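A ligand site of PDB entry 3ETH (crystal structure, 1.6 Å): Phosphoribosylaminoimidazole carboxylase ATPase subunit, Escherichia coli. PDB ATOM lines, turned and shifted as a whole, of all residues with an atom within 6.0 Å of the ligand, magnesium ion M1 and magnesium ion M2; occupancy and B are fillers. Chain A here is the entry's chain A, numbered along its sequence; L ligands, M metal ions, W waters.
OE2 of Glu 226 lies close to NE2 of His 244 (3.2 Å).
OE2 of Glu 238 lies close to NH1 of Arg 80 (3.1 Å).
The side-chain hydroxyl (OH) of Tyr 126 sits close to the guanidinium group (NE) of Arg 129, at 3.1 Å.
OE2 of Glu 153 is in salt-bridge range of NZ of Lys 120 (3.2 Å).
A ring nitrogen (ND1) of His 184 is in hydrogen-bond range of the side-chain carboxylate (OE1) of Glu 161, at 2.9 Å.
The backbone NH (N) of Glu 153 is in hydrogen-bond range of the backbone carbonyl oxygen (O) of Ile 118, 2.6 Å away.
N of Asn 237 is in hydrogen-bond range of O of Glu 226 (2.7 Å).
The side-chain carboxylate of Asp 127 lies within salt-bridge range of the side-chain amino group of Lys 314, 3.6 Å away.
Residues that only touch magnesium ion M2: Arg 80 (3.99 Å).
Two residues have an atom within 4 Å of magnesium ion M2: Arg 80 and Glu 238.
Magnesium ion M1 is bound by the side-chain carboxylate (OE1) of Glu 238 (2.0 Å), an oxygen (O1) of the ligand (2.0 Å), an oxygen (O8) of the ligand (2.0 Å), water W6 (2.1 Å), the side-chain carboxylate (OE1) of Glu 226 (2.1 Å) and the side-chain carboxylate (OE2) of Glu 226 (2.3 Å).
Magnesium ion M1 has six donor atoms within binding distance.
Residues that only touch magnesium ion M1: Asn 237.
Three residues have an atom within 4 Å of magnesium ion M1: Glu 226, Asn 237 and Glu 238.
Along chain A the residues within 4 Å of magnesium ion M1 span positions 226 to 238.
Water W6 lies within hydrogen-bond range of an oxygen (O12) of the ligand and a ring nitrogen (NE2) of His 184.
Water W8 lies within hydrogen-bond range of O of Gly 125 and NH2 of Arg 80.
Water W5 lies within hydrogen-bond range of the backbone carbonyl oxygen of Gly 187 (2.8 Å) and an oxygen (O6) of the ligand (3.2 Å).
Water W7 bridges O3 of the ligand (3.0 Å) and NZ of Lys 314 (3.5 Å).
Water W2 lies within hydrogen-bond range of the side-chain amide nitrogen of Gln 131 (2.6 Å) and an oxygen (O9) of the ligand (3.2 Å).
Magnesium ion M2 is bound by O2 of the ligand (1.9 Å), O5 of the ligand (1.9 Å), OE1 of Glu 238 (2.1 Å), water W8 (2.1 Å), water W4 (2.1 Å) and OE2 of Glu 238 (2.2 Å).
Residues that only touch the ligand: Ile 118, Gly 125, Gly 155, Phe 158 and Phe 228.
Within 4 Å of the ligand: Arg 80, Ile 118, Lys 120, Gly 125, Tyr 126, Asp 127, Gly 128, Gln 131, Glu 153, Gln 154, Gly 155, Ile 156, Phe 158, Glu 161, His 184, Glu 226, Phe 228, Asn 237 and Glu 238.
An oxygen (O4) of the ligand lies within hydrogen-bond range of the backbone NH of Gly 128 (2.8 Å).
O3 of the ligand lies within hydrogen-bond range of N of Asp 127, at 2.6 Å.
N of Ile 156 is in hydrogen-bond range of N4 of the ligand, at 2.9 Å.
The backbone NH (N) of Tyr 126 sits close to an oxygen (O4) of the ligand (3.1 Å).
The side-chain carboxylate of Glu 161 lies within hydrogen-bond range of an oxygen (O12) of the ligand, at 2.5 Å.
NH1 of Arg 80 lies within salt-bridge range of O7 of the ligand, at 3.7 Å.
N3 of the ligand is in hydrogen-bond range of O of Gln 154 (3.0 Å).
NE2 of Gln 131 is in hydrogen-bond range of O10 of the ligand, 3.1 Å away.
The side-chain carboxylate (OE2) of Glu 153 is in hydrogen-bond range of a nitrogen (N3) of the ligand, 3.0 Å away.
The side-chain amino group (NZ) of Lys 120 lies within salt-bridge range of an oxygen (O7) of the ligand (2.7 Å).
O12 of the ligand is in hydrogen-bond range of ND1 of His 184 (3.4 Å).
ND2 of Asn 237 lies close to O8 of the ligand (3.1 Å).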
ATOM      1  N   ARG A  80      -9.674 -15.742 -23.108  1.00  0.00           N
ATOM      2  CA  ARG A  80     -10.019 -17.147 -22.837  1.00  0.00           C
ATOM      3  C   ARG A  80     -11.490 -17.485 -23.174  1.00  0.00           C
ATOM      4  O   ARG A  80     -11.833 -18.607 -23.618  1.00  0.00           O
ATOM      5  CB  ARG A  80      -9.733 -17.491 -21.376  1.00  0.00           C
ATOM      6  CG  ARG A  80      -8.271 -17.411 -20.966  1.00  0.00           C
ATOM      7  CD  ARG A  80      -8.001 -18.233 -19.681  1.00  0.00           C
ATOM      8  NE  ARG A  80      -6.654 -17.895 -19.179  1.00  0.00           N
ATOM      9  CZ  ARG A  80      -5.566 -18.589 -19.501  1.00  0.00           C
ATOM     10  NH1 ARG A  80      -5.681 -19.645 -20.289  1.00  0.00           N
ATOM     11  NH2 ARG A  80      -4.364 -18.235 -19.071  1.00  0.00           N
ATOM     12  N   ALA A  95     -12.157 -28.694 -21.271  1.00  0.00           N
ATOM     13  CA  ALA A  95     -12.803 -28.691 -19.953  1.00  0.00           C
ATOM     14  C   ALA A  95     -14.096 -27.908 -19.961  1.00  0.00           C
ATOM     15  O   ALA A  95     -14.127 -26.781 -20.425  1.00  0.00           O
ATOM     16  CB  ALA A  95     -11.882 -28.029 -18.934  1.00  0.00           C
ATOM     17  N   ILE A 118     -11.510 -24.217 -11.492  1.00  0.00           N
ATOM     18  CA  ILE A 118     -10.271 -23.575 -11.882  1.00  0.00           C
ATOM     19  C   ILE A 118     -10.734 -22.317 -12.568  1.00  0.00           C
ATOM     20  O   ILE A 118     -11.318 -22.326 -13.668  1.00  0.00           O
ATOM     21  CB  ILE A 118      -9.473 -24.397 -12.966  1.00  0.00           C
ATOM     22  CG1 ILE A 118      -9.355 -25.924 -12.658  1.00  0.00           C
ATOM     23  CG2 ILE A 118      -8.126 -23.724 -13.260  1.00  0.00           C
ATOM     24  CD1 ILE A 118      -8.838 -26.265 -11.270  1.00  0.00           C
ATOM     25  N   LYS A 120      -9.740 -18.717 -14.122  1.00  0.00           N
ATOM     26  CA  LYS A 120      -8.693 -18.095 -14.942  1.00  0.00           C
ATOM     27  C   LYS A 120      -9.099 -16.735 -15.524  1.00  0.00           C
ATOM     28  O   LYS A 120     -10.152 -16.621 -16.154  1.00  0.00           O
ATOM     29  CB  LYS A 120      -8.352 -19.008 -16.114  1.00  0.00           C
ATOM     30  CG  LYS A 120      -8.072 -20.477 -15.806  1.00  0.00           C
ATOM     31  CD  LYS A 120      -7.563 -21.178 -17.075  1.00  0.00           C
ATOM     32  CE  LYS A 120      -7.278 -22.621 -16.805  1.00  0.00           C
ATOM     33  NZ  LYS A 120      -6.608 -23.386 -17.945  1.00  0.00           N
ATOM     34  N   GLY A 125      -3.008 -13.827 -18.521  1.00  0.00           N
ATOM     35  CA  GLY A 125      -2.366 -14.819 -17.675  1.00  0.00           C
ATOM     36  C   GLY A 125      -1.217 -15.553 -18.357  1.00  0.00           C
ATOM     37  O   GLY A 125      -1.197 -15.757 -19.582  1.00  0.00           O
ATOM     38  N   TYR A 126      -0.228 -15.925 -17.555  1.00  0.00           N
ATOM     39  CA  TYR A 126       0.879 -16.717 -18.058  1.00  0.00           C
ATOM     40  C   TYR A 126       1.450 -17.350 -16.783  1.00  0.00           C
ATOM     41  O   TYR A 126       1.263 -16.851 -15.653  1.00  0.00           O
ATOM     42  CB  TYR A 126       1.920 -15.918 -18.868  1.00  0.00           C
ATOM     43  CG  TYR A 126       2.598 -14.801 -18.079  1.00  0.00           C
ATOM     44  CD1 TYR A 126       3.776 -15.007 -17.393  1.00  0.00           C
ATOM     45  CD2 TYR A 126       2.005 -13.554 -17.992  1.00  0.00           C
ATOM     46  CE1 TYR A 126       4.368 -14.003 -16.670  1.00  0.00           C
ATOM     47  CE2 TYR A 126       2.590 -12.549 -17.275  1.00  0.00           C
ATOM     48  CZ  TYR A 126       3.779 -12.756 -16.641  1.00  0.00           C
ATOM     49  OH  TYR A 126       4.313 -11.678 -15.949  1.00  0.00           O
ATOM     50  N   ASP A 127       2.162 -18.452 -16.993  1.00  0.00           N
ATOM     51  CA  ASP A 127       2.757 -19.178 -15.887  1.00  0.00           C
ATOM     52  C   ASP A 127       1.801 -19.404 -14.693  1.00  0.00           C
ATOM     53  O   ASP A 127       2.273 -19.516 -13.549  1.00  0.00           O
ATOM     54  CB  ASP A 127       4.019 -18.459 -15.359  1.00  0.00           C
ATOM     55  CG  ASP A 127       5.130 -18.448 -16.361  1.00  0.00           C
ATOM     56  OD1 ASP A 127       5.062 -19.339 -17.217  1.00  0.00           O
ATOM     57  OD2 ASP A 127       6.001 -17.556 -16.325  1.00  0.00           O
ATOM     58  N   GLY A 128       0.489 -19.478 -14.912  1.00  0.00           N
ATOM     59  CA  GLY A 128      -0.411 -19.727 -13.768  1.00  0.00           C
ATOM     60  C   GLY A 128      -0.778 -18.478 -12.944  1.00  0.00           C
ATOM     61  O   GLY A 128      -1.517 -18.565 -11.945  1.00  0.00           O
ATOM     62  N   ARG A 129      -0.265 -17.310 -13.311  1.00  0.00           N
ATOM     63  CA  ARG A 129      -0.641 -16.113 -12.534  1.00  0.00           C
ATOM     64  C   ARG A 129      -2.081 -15.849 -12.954  1.00  0.00           C
ATOM     65  O   ARG A 129      -2.420 -16.062 -14.117  1.00  0.00           O
ATOM     66  CB  ARG A 129       0.202 -14.891 -12.916  1.00  0.00           C
ATOM     67  CG  ARG A 129       1.700 -15.143 -12.757  1.00  0.00           C
ATOM     68  CD  ARG A 129       2.576 -14.388 -13.792  1.00  0.00           C
ATOM     69  NE  ARG A 129       2.157 -12.991 -14.101  1.00  0.00           N
ATOM     70  CZ  ARG A 129       2.443 -11.913 -13.365  1.00  0.00           C
ATOM     71  NH1 ARG A 129       3.127 -12.050 -12.233  1.00  0.00           N
ATOM     72  NH2 ARG A 129       2.061 -10.684 -13.748  1.00  0.00           N
ATOM     73  N   GLN A 131      -4.641 -17.437 -11.950  1.00  0.00           N
ATOM     74  CA  GLN A 131      -5.362 -18.696 -11.894  1.00  0.00           C
ATOM     75  C   GLN A 131      -5.647 -19.074 -10.419  1.00  0.00           C
ATOM     76  O   GLN A 131      -4.752 -18.996  -9.571  1.00  0.00           O
ATOM     77  CB  GLN A 131      -4.520 -19.756 -12.608  1.00  0.00           C
ATOM     78  CG  GLN A 131      -5.232 -21.097 -12.574  1.00  0.00           C
ATOM     79  CD  GLN A 131      -4.433 -22.272 -13.115  1.00  0.00           C
ATOM     80  OE1 GLN A 131      -4.143 -23.225 -12.370  1.00  0.00           O
ATOM     81  NE2 GLN A 131      -4.106 -22.220 -14.422  1.00  0.00           N
ATOM     82  N   GLU A 153     -13.287 -23.250 -15.049  1.00  0.00           N
ATOM     83  CA  GLU A 153     -13.383 -24.547 -15.734  1.00  0.00           C
ATOM     84  C   GLU A 153     -13.333 -25.677 -14.729  1.00  0.00           C
ATOM     85  O   GLU A 153     -12.884 -25.498 -13.572  1.00  0.00           O
ATOM     86  CB  GLU A 153     -12.099 -24.911 -16.517  1.00  0.00           C
ATOM     87  CG  GLU A 153     -11.338 -23.801 -17.040  1.00  0.00           C
ATOM     88  CD  GLU A 153     -10.370 -24.330 -18.055  1.00  0.00           C
ATOM     89  OE1 GLU A 153     -10.635 -24.186 -19.285  1.00  0.00           O
ATOM     90  OE2 GLU A 153      -9.372 -24.951 -17.598  1.00  0.00           O
ATOM     91  N   GLN A 154     -13.742 -26.839 -15.206  1.00  0.00           N
ATOM     92  CA  GLN A 154     -13.715 -28.064 -14.411  1.00  0.00           C
ATOM     93  C   GLN A 154     -12.239 -28.425 -14.178  1.00  0.00           C
ATOM     94  O   GLN A 154     -11.397 -28.329 -15.079  1.00  0.00           O
ATOM     95  CB  GLN A 154     -14.384 -29.228 -15.164  1.00  0.00           C
ATOM     96  CG  GLN A 154     -14.572 -30.420 -14.246  1.00  0.00           C
ATOM     97  CD  GLN A 154     -14.417 -31.813 -14.899  1.00  0.00           C
ATOM     98  OE1 GLN A 154     -13.953 -32.758 -14.266  1.00  0.00           O
ATOM     99  NE2 GLN A 154     -14.815 -31.931 -16.142  1.00  0.00           N
ATOM    100  N   GLY A 155     -11.903 -28.846 -12.961  1.00  0.00           N
ATOM    101  CA  GLY A 155     -10.548 -29.268 -12.594  1.00  0.00           C
ATOM    102  C   GLY A 155     -10.375 -30.599 -13.338  1.00  0.00           C
ATOM    103  O   GLY A 155     -11.124 -31.546 -13.098  1.00  0.00           O
ATOM    104  N   ILE A 156      -9.384 -30.688 -14.229  1.00  0.00           N
ATOM    105  CA  ILE A 156      -9.178 -31.951 -14.942  1.00  0.00           C
ATOM    106  C   ILE A 156      -8.094 -32.836 -14.304  1.00  0.00           C
ATOM    107  O   ILE A 156      -6.976 -32.417 -14.063  1.00  0.00           O
ATOM    108  CB  ILE A 156      -8.810 -31.713 -16.430  1.00  0.00           C
ATOM    109  CG1 ILE A 156      -9.895 -30.890 -17.146  1.00  0.00           C
ATOM    110  CG2 ILE A 156      -8.600 -33.053 -17.159  1.00  0.00           C
ATOM    111  CD1 ILE A 156     -11.343 -31.477 -17.084  1.00  0.00           C
ATOM    112  N   ASN A 157      -8.391 -34.110 -14.052  1.00  0.00           N
ATOM    113  CA  ASN A 157      -7.332 -34.944 -13.477  1.00  0.00           C
ATOM    114  C   ASN A 157      -6.637 -35.726 -14.602  1.00  0.00           C
ATOM    115  O   ASN A 157      -6.868 -36.902 -14.897  1.00  0.00           O
ATOM    116  CB  ASN A 157      -7.818 -35.807 -12.299  1.00  0.00           C
ATOM    117  CG  ASN A 157      -9.233 -35.447 -11.892  1.00  0.00           C
ATOM    118  OD1 ASN A 157      -9.506 -34.339 -11.419  1.00  0.00           O
ATOM    119  ND2 ASN A 157     -10.159 -36.379 -12.119  1.00  0.00           N
ATOM    120  N   PHE A 158      -5.753 -35.036 -15.284  1.00  0.00           N
ATOM    121  CA  PHE A 158      -5.070 -35.715 -16.378  1.00  0.00           C
ATOM    122  C   PHE A 158      -3.918 -36.606 -15.858  1.00  0.00           C
ATOM    123  O   PHE A 158      -3.383 -36.454 -14.758  1.00  0.00           O
ATOM    124  CB  PHE A 158      -4.580 -34.617 -17.324  1.00  0.00           C
ATOM    125  CG  PHE A 158      -3.820 -33.533 -16.605  1.00  0.00           C
ATOM    126  CD1 PHE A 158      -4.427 -32.313 -16.305  1.00  0.00           C
ATOM    127  CD2 PHE A 158      -2.480 -33.731 -16.262  1.00  0.00           C
ATOM    128  CE1 PHE A 158      -3.692 -31.317 -15.684  1.00  0.00           C
ATOM    129  CE2 PHE A 158      -1.725 -32.752 -15.673  1.00  0.00           C
ATOM    130  CZ  PHE A 158      -2.344 -31.527 -15.355  1.00  0.00           C
ATOM    131  N   GLU A 161       0.561 -34.096 -19.402  1.00  0.00           N
ATOM    132  CA  GLU A 161       0.276 -32.956 -20.274  1.00  0.00           C
ATOM    133  C   GLU A 161       1.107 -33.026 -21.550  1.00  0.00           C
ATOM    134  O   GLU A 161       2.278 -33.424 -21.498  1.00  0.00           O
ATOM    135  CB  GLU A 161       0.646 -31.671 -19.531  1.00  0.00           C
ATOM    136  CG  GLU A 161      -0.364 -31.391 -18.395  1.00  0.00           C
ATOM    137  CD  GLU A 161      -0.202 -29.949 -17.897  1.00  0.00           C
ATOM    138  OE1 GLU A 161       0.349 -29.783 -16.801  1.00  0.00           O
ATOM    139  OE2 GLU A 161      -0.638 -28.977 -18.567  1.00  0.00           O
ATOM    140  N   HIS A 184       4.764 -29.204 -15.557  1.00  0.00           N
ATOM    141  CA  HIS A 184       4.609 -27.859 -14.980  1.00  0.00           C
ATOM    142  C   HIS A 184       4.587 -27.962 -13.468  1.00  0.00           C
ATOM    143  O   HIS A 184       3.964 -28.837 -12.889  1.00  0.00           O
ATOM    144  CB  HIS A 184       3.280 -27.168 -15.389  1.00  0.00           C
ATOM    145  CG  HIS A 184       3.098 -27.070 -16.870  1.00  0.00           C
ATOM    146  ND1 HIS A 184       2.530 -28.085 -17.612  1.00  0.00           N
ATOM    147  CD2 HIS A 184       3.493 -26.110 -17.745  1.00  0.00           C
ATOM    148  CE1 HIS A 184       2.561 -27.740 -18.896  1.00  0.00           C
ATOM    149  NE2 HIS A 184       3.110 -26.534 -18.991  1.00  0.00           N
ATOM    150  N   GLY A 187       2.562 -23.780 -11.623  1.00  0.00           N
ATOM    151  CA  GLY A 187       2.061 -23.069 -12.779  1.00  0.00           C
ATOM    152  C   GLY A 187       3.030 -22.786 -13.914  1.00  0.00           C
ATOM    153  O   GLY A 187       2.569 -22.367 -14.950  1.00  0.00           O
ATOM    154  N   ILE A 188       4.332 -22.984 -13.746  1.00  0.00           N
ATOM    155  CA  ILE A 188       5.264 -22.712 -14.847  1.00  0.00           C
ATOM    156  C   ILE A 188       5.875 -23.994 -15.445  1.00  0.00           C
ATOM    157  O   ILE A 188       6.153 -24.967 -14.721  1.00  0.00           O
ATOM    158  CB  ILE A 188       6.381 -21.760 -14.312  1.00  0.00           C
ATOM    159  CG1 ILE A 188       7.485 -21.437 -15.356  1.00  0.00           C
ATOM    160  CG2 ILE A 188       7.074 -22.421 -13.146  1.00  0.00           C
ATOM    161  CD1 ILE A 188       7.962 -19.973 -15.407  1.00  0.00           C
ATOM    162  N   GLU A 226      -1.732 -26.815 -26.127  1.00  0.00           N
ATOM    163  CA  GLU A 226      -1.487 -27.506 -24.861  1.00  0.00           C
ATOM    164  C   GLU A 226      -2.768 -28.318 -24.591  1.00  0.00           C
ATOM    165  O   GLU A 226      -3.908 -27.813 -24.694  1.00  0.00           O
ATOM    166  CB  GLU A 226      -1.355 -26.562 -23.686  1.00  0.00           C
ATOM    167  CG  GLU A 226      -0.168 -25.561 -23.815  1.00  0.00           C
ATOM    168  CD  GLU A 226      -0.136 -24.676 -22.570  1.00  0.00           C
ATOM    169  OE1 GLU A 226      -1.056 -24.761 -21.713  1.00  0.00           O
ATOM    170  OE2 GLU A 226       0.795 -23.870 -22.417  1.00  0.00           O
ATOM    171  N   PHE A 228      -4.464 -31.882 -22.326  1.00  0.00           N
ATOM    172  CA  PHE A 228      -4.460 -32.755 -21.154  1.00  0.00           C
ATOM    173  C   PHE A 228      -4.798 -34.161 -21.675  1.00  0.00           C
ATOM    174  O   PHE A 228      -5.721 -34.335 -22.493  1.00  0.00           O
ATOM    175  CB  PHE A 228      -5.616 -32.344 -20.233  1.00  0.00           C
ATOM    176  CG  PHE A 228      -5.418 -31.023 -19.553  1.00  0.00           C
ATOM    177  CD1 PHE A 228      -4.135 -30.474 -19.378  1.00  0.00           C
ATOM    178  CD2 PHE A 228      -6.521 -30.319 -19.084  1.00  0.00           C
ATOM    179  CE1 PHE A 228      -3.961 -29.278 -18.731  1.00  0.00           C
ATOM    180  CE2 PHE A 228      -6.368 -29.104 -18.423  1.00  0.00           C
ATOM    181  CZ  PHE A 228      -5.072 -28.575 -18.251  1.00  0.00           C
ATOM    182  N   ASN A 237      -6.272 -27.585 -23.448  1.00  0.00           N
ATOM    183  CA  ASN A 237      -6.208 -26.688 -22.301  1.00  0.00           C
ATOM    184  C   ASN A 237      -6.202 -25.250 -22.855  1.00  0.00           C
ATOM    185  O   ASN A 237      -7.082 -24.450 -22.523  1.00  0.00           O
ATOM    186  CB  ASN A 237      -4.943 -26.962 -21.467  1.00  0.00           C
ATOM    187  CG  ASN A 237      -4.645 -25.892 -20.430  1.00  0.00           C
ATOM    188  OD1 ASN A 237      -5.567 -25.466 -19.725  1.00  0.00           O
ATOM    189  ND2 ASN A 237      -3.369 -25.482 -20.278  1.00  0.00           N
ATOM    190  N   GLU A 238      -5.210 -24.927 -23.683  1.00  0.00           N
ATOM    191  CA  GLU A 238      -5.088 -23.574 -24.237  1.00  0.00           C
ATOM    192  C   GLU A 238      -4.172 -23.515 -25.463  1.00  0.00           C
ATOM    193  O   GLU A 238      -3.462 -24.487 -25.797  1.00  0.00           O
ATOM    194  CB  GLU A 238      -4.650 -22.612 -23.133  1.00  0.00           C
ATOM    195  CG  GLU A 238      -3.143 -22.727 -22.812  1.00  0.00           C
ATOM    196  CD  GLU A 238      -2.520 -21.507 -22.109  1.00  0.00           C
ATOM    197  OE1 GLU A 238      -1.390 -21.614 -21.590  1.00  0.00           O
ATOM    198  OE2 GLU A 238      -3.180 -20.442 -21.997  1.00  0.00           O
ATOM    199  N   LEU A 239      -4.226 -22.409 -26.162  1.00  0.00           N
ATOM    200  CA  LEU A 239      -3.425 -22.239 -27.368  1.00  0.00           C
ATOM    201  C   LEU A 239      -2.502 -21.031 -27.176  1.00  0.00           C
ATOM    202  O   LEU A 239      -2.889 -20.087 -26.483  1.00  0.00           O
ATOM    203  CB  LEU A 239      -4.284 -21.780 -28.579  1.00  0.00           C
ATOM    204  CG  LEU A 239      -5.585 -22.507 -28.927  1.00  0.00           C
ATOM    205  CD1 LEU A 239      -6.233 -21.929 -30.167  1.00  0.00           C
ATOM    206  CD2 LEU A 239      -5.161 -23.918 -29.248  1.00  0.00           C
ATOM    207  N   ARG A 242       1.899 -18.614 -31.522  1.00  0.00           N
ATOM    208  CA  ARG A 242       3.286 -18.270 -31.753  1.00  0.00           C
ATOM    209  C   ARG A 242       4.104 -19.484 -31.403  1.00  0.00           C
ATOM    210  O   ARG A 242       3.533 -20.438 -30.927  1.00  0.00           O
ATOM    211  CB  ARG A 242       3.702 -17.209 -30.695  1.00  0.00           C
ATOM    212  CG  ARG A 242       3.198 -17.505 -29.265  1.00  0.00           C
ATOM    213  CD  ARG A 242       3.865 -16.647 -28.224  1.00  0.00           C
ATOM    214  NE  ARG A 242       3.220 -16.799 -26.925  1.00  0.00           N
ATOM    215  CZ  ARG A 242       3.500 -17.763 -26.042  1.00  0.00           C
ATOM    216  NH1 ARG A 242       4.386 -18.719 -26.330  1.00  0.00           N
ATOM    217  NH2 ARG A 242       2.881 -17.751 -24.852  1.00  0.00           N
ATOM    218  N   HIS A 244       6.472 -21.583 -29.018  1.00  0.00           N
ATOM    219  CA  HIS A 244       6.122 -21.802 -27.627  1.00  0.00           C
ATOM    220  C   HIS A 244       7.223 -22.491 -26.848  1.00  0.00           C
ATOM    221  O   HIS A 244       7.962 -23.291 -27.417  1.00  0.00           O
ATOM    222  CB  HIS A 244       4.826 -22.678 -27.697  1.00  0.00           C
ATOM    223  CG  HIS A 244       4.216 -22.992 -26.360  1.00  0.00           C
ATOM    224  ND1 HIS A 244       4.507 -24.141 -25.641  1.00  0.00           N
ATOM    225  CD2 HIS A 244       3.263 -22.331 -25.655  1.00  0.00           C
ATOM    226  CE1 HIS A 244       3.785 -24.156 -24.533  1.00  0.00           C
ATOM    227  NE2 HIS A 244       3.005 -23.072 -24.528  1.00  0.00           N
ATOM    228  N   LYS A 314      11.934 -16.902 -16.512  1.00  0.00           N
ATOM    229  CA  LYS A 314      12.637 -17.776 -17.409  1.00  0.00           C
ATOM    230  C   LYS A 314      13.887 -17.031 -17.891  1.00  0.00           C
ATOM    231  O   LYS A 314      13.846 -15.964 -18.560  1.00  0.00           O
ATOM    232  CB  LYS A 314      11.764 -18.108 -18.621  1.00  0.00           C
ATOM    233  CG  LYS A 314      10.493 -18.855 -18.180  1.00  0.00           C
ATOM    234  CD  LYS A 314       9.514 -19.096 -19.332  1.00  0.00           C
ATOM    235  CE  LYS A 314       8.413 -20.015 -18.822  1.00  0.00           C
ATOM    236  NZ  LYS A 314       7.390 -20.262 -19.858  1.00  0.00           N
HETATM  237  P1  LIG L   1       1.019 -20.346 -19.694  1.00  0.00           P
HETATM  238  O1  LIG L   1       1.101 -21.766 -20.244  1.00  0.00           O
HETATM  239  O2  LIG L   1       0.475 -19.303 -20.767  1.00  0.00           O
HETATM  240  O3  LIG L   1       2.336 -19.890 -19.171  1.00  0.00           O
HETATM  241  P2  LIG L   1      -1.278 -19.936 -18.188  1.00  0.00           P
HETATM  242  O4  LIG L   1      -1.167 -18.845 -17.104  1.00  0.00           O
HETATM  243  O5  LIG L   1      -1.912 -19.597 -19.510  1.00  0.00           O
HETATM  244  O6  LIG L   1       0.106 -20.640 -18.410  1.00  0.00           O
HETATM  245  P3  LIG L   1      -2.635 -22.530 -18.028  1.00  0.00           P
HETATM  246  O7  LIG L   1      -4.113 -22.291 -18.253  1.00  0.00           O
HETATM  247  O8  LIG L   1      -1.945 -22.865 -19.307  1.00  0.00           O
HETATM  248  O9  LIG L   1      -2.142 -21.092 -17.535  1.00  0.00           O
HETATM  249  O10 LIG L   1      -2.383 -23.409 -16.687  1.00  0.00           O
HETATM  250  C1  LIG L   1      -1.036 -23.784 -16.233  1.00  0.00           C
HETATM  251  C2  LIG L   1      -1.052 -25.270 -15.865  1.00  0.00           C
HETATM  252  O11 LIG L   1      -2.122 -25.390 -14.901  1.00  0.00           O
HETATM  253  C3  LIG L   1      -1.563 -26.251 -16.935  1.00  0.00           C
HETATM  254  O12 LIG L   1      -0.510 -26.616 -17.844  1.00  0.00           O
HETATM  255  C4  LIG L   1      -1.964 -27.415 -16.022  1.00  0.00           C
HETATM  256  O13 LIG L   1      -0.837 -27.915 -15.331  1.00  0.00           O
HETATM  257  C5  LIG L   1      -2.696 -26.667 -14.919  1.00  0.00           C
HETATM  258  N1  LIG L   1      -4.102 -26.508 -15.294  1.00  0.00           N
HETATM  259  C6  LIG L   1      -4.645 -25.488 -16.015  1.00  0.00           C
HETATM  260  N2  LIG L   1      -5.956 -25.695 -16.199  1.00  0.00           N
HETATM  261  C7  LIG L   1      -6.286 -26.896 -15.553  1.00  0.00           C
HETATM  262  C8  LIG L   1      -7.536 -27.581 -15.384  1.00  0.00           C
HETATM  263  N3  LIG L   1      -8.663 -27.208 -15.806  1.00  0.00           N
HETATM  264  N4  LIG L   1      -7.347 -28.690 -14.600  1.00  0.00           N
HETATM  265  C9  LIG L   1      -6.169 -29.120 -14.063  1.00  0.00           C
HETATM  266  N5  LIG L   1      -5.024 -28.523 -14.213  1.00  0.00           N
HETATM  267  C10 LIG L   1      -5.132 -27.391 -14.955  1.00  0.00           C
HETATM  268 MG    MG M   1      -0.420 -23.050 -20.653  1.00  0.00          MG
HETATM  269 MG    MG M   2      -1.297 -19.530 -21.273  1.00  0.00          MG
HETATM  270  O   HOH W   1       3.496 -23.035 -20.910  1.00  0.00           O
HETATM  271  O   HOH W   2      -4.743 -20.201 -15.901  1.00  0.00           O
HETATM  272  O   HOH W   3       1.484 -21.095 -23.034  1.00  0.00           O
HETATM  273  O   HOH W   4      -0.775 -19.383 -23.333  1.00  0.00           O
HETATM  274  O   HOH W   5       2.295 -22.877 -17.733  1.00  0.00           O
HETATM  275  O   HOH W   6       0.760 -24.222 -19.371  1.00  0.00           O
HETATM  276  O   HOH W   7       4.508 -18.443 -20.653  1.00  0.00           O
HETATM  277  O   HOH W   8      -2.025 -17.549 -21.418  1.00  0.00           O
